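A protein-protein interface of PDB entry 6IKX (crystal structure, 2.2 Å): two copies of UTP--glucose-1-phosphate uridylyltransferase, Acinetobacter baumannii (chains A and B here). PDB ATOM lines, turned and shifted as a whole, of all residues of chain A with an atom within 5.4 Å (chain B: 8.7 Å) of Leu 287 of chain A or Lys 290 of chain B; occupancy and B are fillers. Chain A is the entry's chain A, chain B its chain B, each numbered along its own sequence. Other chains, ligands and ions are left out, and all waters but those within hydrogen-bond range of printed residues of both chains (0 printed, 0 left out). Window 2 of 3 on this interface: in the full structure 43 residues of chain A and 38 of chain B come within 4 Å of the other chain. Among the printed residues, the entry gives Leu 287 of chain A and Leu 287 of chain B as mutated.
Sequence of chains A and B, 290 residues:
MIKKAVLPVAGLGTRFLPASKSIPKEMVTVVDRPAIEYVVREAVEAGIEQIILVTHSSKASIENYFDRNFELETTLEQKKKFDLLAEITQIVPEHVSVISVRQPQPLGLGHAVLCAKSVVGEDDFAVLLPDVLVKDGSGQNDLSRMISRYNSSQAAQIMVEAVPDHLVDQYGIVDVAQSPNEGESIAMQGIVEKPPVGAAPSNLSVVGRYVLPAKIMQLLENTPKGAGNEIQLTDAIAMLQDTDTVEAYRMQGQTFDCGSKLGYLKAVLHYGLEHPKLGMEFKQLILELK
Of the 8 printed residues of chain B, 3 touch a printed residue of chain A.
Hydrophobic or aromatic side chains of chain B that line the printed part of chain A: Leu 269 and Leu 289.
Of the 9 printed residues of chain A, 5 touch a printed residue of chain B.
Hydrophobic or aromatic side chains of chain A within 4 Å of the printed part of chain B: Leu 273, Leu 285, Ile 286 and Leu 287.
Among the printed residues, 6 pairs touch across the chains.
Among the printed residues, merely in contact across the chains: Leu 273 of chain A with Leu 289 of chain B (3.8 Å), Leu 273 of chain A with Lys 290 of chain B (3.9 Å), Lys 283 of chain A with Lys 290 of chain B (3.6 Å), Leu 285 of chain A with Leu 269 of chain B (3.7 Å), Ile 286 of chain A with Leu 269 of chain B (3.8 Å) and Leu 287 of chain A with Lys 290 of chain B (3.8 Å).
Leu 287 of chain A touches Lys 290 of chain B, but with the chains exchanged Lys 290 of chain A does not touch Leu 287 of chain B (4.5 Å).
Positions printed for both chains: 284, 285, 286, 287, 288, 289 and 290.
Of the 6 pairs that touch across the chains among the printed residues, none has its exchanged pair printed and touching as well.
Of the printed residues of chain B, Lys 283 of chain A touches Lys 290 (3.6 Å).
Of the printed residues of chain B, Leu 287 of chain A touches Lys 290 (3.8 Å).
Printed residues of chain A within 4 Å of Leu 269 of chain B: Leu 285 (3.7 Å) and Ile 286 (3.8 Å).
Printed residues of chain A within 4 Å of Leu 289 of chain B: Leu 273 (3.8 Å).
Lys 290 of chain B touches just these residues of chain A: Leu 273, Lys 283 and Leu 287.
The nearest printed residue of chain B that does not touch Leu 287 of chain A is Ile 286 of chain B (6.7 Å).
The nearest printed residue of chain A that does not touch Lys 290 of chain B is Ile 286 of chain A (5.4 Å).
The nearest printed residue of chain A that does not touch Leu 289 of chain B is Ile 286 of chain A (4.9 Å).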
ATOM      1  N   LEU A 273     -11.075 -13.223 -36.727  1.00  0.00           N
ATOM      2  CA  LEU A 273     -10.520 -11.846 -36.907  1.00  0.00           C
ATOM      3  C   LEU A 273     -10.109 -11.608 -38.365  1.00  0.00           C
ATOM      4  O   LEU A 273     -10.218 -10.470 -38.827  1.00  0.00           O
ATOM      5  CB  LEU A 273      -9.346 -11.624 -35.950  1.00  0.00           C
ATOM      6  CG  LEU A 273      -9.726 -11.031 -34.588  1.00  0.00           C
ATOM      7  CD2 LEU A 273      -8.621 -11.266 -33.582  1.00  0.00           C
ATOM      8  N   LYS A 283     -13.990  -8.187 -34.164  1.00  0.00           N
ATOM      9  CA  LYS A 283     -13.014  -7.404 -33.355  1.00  0.00           C
ATOM     10  C   LYS A 283     -13.765  -6.599 -32.283  1.00  0.00           C
ATOM     11  O   LYS A 283     -13.429  -6.724 -31.074  1.00  0.00           O
ATOM     12  CB  LYS A 283     -12.222  -6.484 -34.290  1.00  0.00           C
ATOM     13  CG  LYS A 283     -11.054  -5.721 -33.675  1.00  0.00           C
ATOM     14  CD  LYS A 283     -10.800  -4.374 -34.335  1.00  0.00           C
ATOM     15  CE  LYS A 283      -9.371  -4.176 -34.799  1.00  0.00           C
ATOM     16  NZ  LYS A 283      -9.287  -3.025 -35.733  1.00  0.00           N
ATOM     17  N   GLN A 284     -14.750  -5.819 -32.719  1.00  0.00           N
ATOM     18  CA  GLN A 284     -15.657  -4.984 -31.876  1.00  0.00           C
ATOM     19  C   GLN A 284     -16.267  -5.851 -30.751  1.00  0.00           C
ATOM     20  O   GLN A 284     -16.251  -5.421 -29.572  1.00  0.00           O
ATOM     21  CB  GLN A 284     -16.692  -4.323 -32.803  1.00  0.00           C
ATOM     22  CG  GLN A 284     -17.786  -3.517 -32.110  1.00  0.00           C
ATOM     23  CD  GLN A 284     -17.258  -2.275 -31.430  1.00  0.00           C
ATOM     24  OE1 GLN A 284     -16.215  -1.734 -31.797  1.00  0.00           O
ATOM     25  NE2 GLN A 284     -17.973  -1.815 -30.416  1.00  0.00           N
ATOM     26  N   LEU A 285     -16.781  -7.038 -31.078  1.00  0.00           N
ATOM     27  CA  LEU A 285     -17.408  -7.930 -30.077  1.00  0.00           C
ATOM     28  C   LEU A 285     -16.404  -8.210 -28.965  1.00  0.00           C
ATOM     29  O   LEU A 285     -16.845  -8.303 -27.808  1.00  0.00           O
ATOM     30  CB  LEU A 285     -17.834  -9.249 -30.722  1.00  0.00           C
ATOM     31  CG  LEU A 285     -19.152  -9.211 -31.474  1.00  0.00           C
ATOM     32  CD1 LEU A 285     -19.522 -10.617 -31.942  1.00  0.00           C
ATOM     33  CD2 LEU A 285     -20.256  -8.606 -30.608  1.00  0.00           C
ATOM     34  N   ILE A 286     -15.135  -8.429 -29.331  1.00  0.00           N
ATOM     35  CA  ILE A 286     -14.044  -8.812 -28.389  1.00  0.00           C
ATOM     36  C   ILE A 286     -13.746  -7.617 -27.482  1.00  0.00           C
ATOM     37  O   ILE A 286     -13.613  -7.830 -26.274  1.00  0.00           O
ATOM     38  CB  ILE A 286     -12.795  -9.271 -29.159  1.00  0.00           C
ATOM     39  CG1 ILE A 286     -12.896 -10.758 -29.487  1.00  0.00           C
ATOM     40  CD1 ILE A 286     -12.173 -11.144 -30.739  1.00  0.00           C
ATOM     41  N   LEU A 287     -13.650  -6.418 -28.062  1.00  0.00           N
ATOM     42  CA  LEU A 287     -13.318  -5.152 -27.349  1.00  0.00           C
ATOM     43  C   LEU A 287     -14.388  -4.868 -26.283  1.00  0.00           C
ATOM     44  O   LEU A 287     -14.022  -4.658 -25.105  1.00  0.00           O
ATOM     45  CB  LEU A 287     -13.217  -4.027 -28.382  1.00  0.00           C
ATOM     46  CG  LEU A 287     -12.148  -4.221 -29.461  1.00  0.00           C
ATOM     47  CD1 LEU A 287     -10.743  -4.245 -28.880  1.00  0.00           C
ATOM     48  N   GLU A 288     -15.658  -4.928 -26.683  1.00  0.00           N
ATOM     49  CA  GLU A 288     -16.854  -4.881 -25.794  1.00  0.00           C
ATOM     50  C   GLU A 288     -16.724  -5.835 -24.590  1.00  0.00           C
ATOM     51  O   GLU A 288     -17.395  -5.584 -23.573  1.00  0.00           O
ATOM     52  CB  GLU A 288     -18.114  -5.235 -26.589  1.00  0.00           C
ATOM     53  CG  GLU A 288     -18.576  -4.165 -27.569  1.00  0.00           C
ATOM     54  CD  GLU A 288     -19.664  -4.636 -28.529  1.00  0.00           C
ATOM     55  OE1 GLU A 288     -20.231  -5.760 -28.325  1.00  0.00           O
ATOM     56  OE2 GLU A 288     -19.949  -3.887 -29.487  1.00  0.00           O
ATOM     57  N   LEU A 289     -15.940  -6.913 -24.671  1.00  0.00           N
ATOM     58  CA  LEU A 289     -15.814  -7.875 -23.541  1.00  0.00           C
ATOM     59  C   LEU A 289     -15.425  -7.090 -22.276  1.00  0.00           C
ATOM     60  O   LEU A 289     -15.844  -7.504 -21.176  1.00  0.00           O
ATOM     61  CB  LEU A 289     -14.801  -8.974 -23.887  1.00  0.00           C
ATOM     62  CG  LEU A 289     -15.262 -10.002 -24.921  1.00  0.00           C
ATOM     63  CD1 LEU A 289     -16.296 -10.932 -24.314  1.00  0.00           C
ATOM     64  N   LYS A 290     -14.651  -6.008 -22.438  1.00  0.00           N
ATOM     65  CA  LYS A 290     -14.465  -4.925 -21.428  1.00  0.00           C
ATOM     66  C   LYS A 290     -14.342  -3.583 -22.162  1.00  0.00           C
ATOM     67  O   LYS A 290     -15.249  -2.757 -22.055  1.00  0.00           O
ATOM     68  CB  LYS A 290     -13.241  -5.132 -20.519  1.00  0.00           C
ATOM     69  CG  LYS A 290     -12.053  -5.858 -21.133  1.00  0.00           C
ATOM     70  CD  LYS A 290     -12.160  -7.341 -20.912  1.00  0.00           C
ATOM     71  CE  LYS A 290     -11.000  -8.152 -21.437  1.00  0.00           C
ATOM     72  NZ  LYS A 290     -11.292  -9.585 -21.205  1.00  0.00           N
ATOM     73  N   LEU B 269     -17.756 -16.319 -27.545  1.00  0.00           N
ATOM     74  CA  LEU B 269     -17.033 -15.445 -26.578  1.00  0.00           C
ATOM     75  C   LEU B 269     -17.637 -15.570 -25.165  1.00  0.00           C
ATOM     76  O   LEU B 269     -16.920 -16.009 -24.251  1.00  0.00           O
ATOM     77  CB  LEU B 269     -17.074 -13.999 -27.074  1.00  0.00           C
ATOM     78  CG  LEU B 269     -16.367 -13.719 -28.405  1.00  0.00           C
ATOM     79  CD1 LEU B 269     -16.768 -12.347 -28.919  1.00  0.00           C
ATOM     80  CD2 LEU B 269     -14.846 -13.808 -28.300  1.00  0.00           C
ATOM     81  N   GLN B 284      -7.169 -15.759 -21.413  1.00  0.00           N
ATOM     82  CA  GLN B 284      -5.734 -15.490 -21.731  1.00  0.00           C
ATOM     83  C   GLN B 284      -5.506 -15.470 -23.257  1.00  0.00           C
ATOM     84  O   GLN B 284      -4.876 -14.482 -23.745  1.00  0.00           O
ATOM     85  CB  GLN B 284      -4.847 -16.478 -20.957  1.00  0.00           C
ATOM     86  CG  GLN B 284      -3.339 -16.312 -21.151  1.00  0.00           C
ATOM     87  CD  GLN B 284      -2.806 -14.903 -20.998  1.00  0.00           C
ATOM     88  OE1 GLN B 284      -3.447 -14.029 -20.393  1.00  0.00           O
ATOM     89  NE2 GLN B 284      -1.610 -14.680 -21.544  1.00  0.00           N
ATOM     90  N   LEU B 285      -5.995 -16.469 -24.008  1.00  0.00           N
ATOM     91  CA  LEU B 285      -5.914 -16.454 -25.503  1.00  0.00           C
ATOM     92  C   LEU B 285      -6.354 -15.090 -26.023  1.00  0.00           C
ATOM     93  O   LEU B 285      -5.676 -14.565 -26.914  1.00  0.00           O
ATOM     94  CB  LEU B 285      -6.801 -17.530 -26.132  1.00  0.00           C
ATOM     95  CG  LEU B 285      -6.255 -18.950 -26.079  1.00  0.00           C
ATOM     96  CD1 LEU B 285      -7.202 -19.918 -26.775  1.00  0.00           C
ATOM     97  CD2 LEU B 285      -4.860 -19.013 -26.697  1.00  0.00           C
ATOM     98  N   ILE B 286      -7.455 -14.527 -25.509  1.00  0.00           N
ATOM     99  CA  ILE B 286      -7.981 -13.222 -26.042  1.00  0.00           C
ATOM    100  C   ILE B 286      -6.973 -12.094 -25.770  1.00  0.00           C
ATOM    101  O   ILE B 286      -6.717 -11.335 -26.699  1.00  0.00           O
ATOM    102  CB  ILE B 286      -9.382 -12.871 -25.497  1.00  0.00           C
ATOM    103  CG1 ILE B 286     -10.433 -13.869 -25.995  1.00  0.00           C
ATOM    104  CG2 ILE B 286      -9.738 -11.429 -25.862  1.00  0.00           C
ATOM    105  CD1 ILE B 286     -11.682 -13.964 -25.162  1.00  0.00           C
ATOM    106  N   LEU B 287      -6.462 -11.982 -24.532  1.00  0.00           N
ATOM    107  CA  LEU B 287      -5.449 -10.962 -24.122  1.00  0.00           C
ATOM    108  C   LEU B 287      -4.234 -11.067 -25.057  1.00  0.00           C
ATOM    109  O   LEU B 287      -3.719 -10.018 -25.506  1.00  0.00           O
ATOM    110  CB  LEU B 287      -5.051 -11.178 -22.653  1.00  0.00           C
ATOM    111  CG  LEU B 287      -6.188 -11.145 -21.623  1.00  0.00           C
ATOM    112  CD1 LEU B 287      -6.786  -9.750 -21.506  1.00  0.00           C
ATOM    113  N   GLU B 288      -3.828 -12.284 -25.408  1.00  0.00           N
ATOM    114  CA  GLU B 288      -2.628 -12.514 -26.259  1.00  0.00           C
ATOM    115  C   GLU B 288      -2.863 -12.047 -27.721  1.00  0.00           C
ATOM    116  O   GLU B 288      -2.034 -12.441 -28.555  1.00  0.00           O
ATOM    117  CB  GLU B 288      -2.219 -13.997 -26.162  1.00  0.00           C
ATOM    118  CG  GLU B 288      -1.677 -14.444 -24.795  1.00  0.00           C
ATOM    119  CD  GLU B 288      -1.369 -15.942 -24.680  1.00  0.00           C
ATOM    120  OE1 GLU B 288      -1.089 -16.552 -25.716  1.00  0.00           O
ATOM    121  OE2 GLU B 288      -1.425 -16.518 -23.567  1.00  0.00           O
ATOM    122  N   LEU B 289      -3.860 -11.186 -28.038  1.00  0.00           N
ATOM    123  CA  LEU B 289      -4.309 -10.869 -29.437  1.00  0.00           C
ATOM    124  C   LEU B 289      -4.116  -9.394 -29.803  1.00  0.00           C
ATOM    125  O   LEU B 289      -3.423  -9.123 -30.806  1.00  0.00           O
ATOM    126  CB  LEU B 289      -5.795 -11.200 -29.628  1.00  0.00           C
ATOM    127  CG  LEU B 289      -6.134 -12.649 -29.962  1.00  0.00           C
ATOM    128  CD2 LEU B 289      -7.631 -12.780 -30.206  1.00  0.00           C
ATOM    129  N   LYS B 290      -4.819  -8.489 -29.114  1.00  0.00           N
ATOM    130  CA  LYS B 290      -5.079  -7.101 -29.596  1.00  0.00           C
ATOM    131  C   LYS B 290      -3.750  -6.363 -29.762  1.00  0.00           C
ATOM    132  O   LYS B 290      -2.907  -6.737 -28.969  1.00  0.00           O
ATOM    133  CB  LYS B 290      -6.017  -6.341 -28.652  1.00  0.00           C
ATOM    134  CG  LYS B 290      -7.482  -6.374 -29.057  1.00  0.00           C
ATOM    135  CD  LYS B 290      -7.731  -5.874 -30.471  1.00  0.00           C
ATOM    136  CE  LYS B 290      -8.508  -6.855 -31.321  1.00  0.00           C
ATOM    137  NZ  LYS B 290      -7.726  -8.079 -31.603  1.00  0.00           N
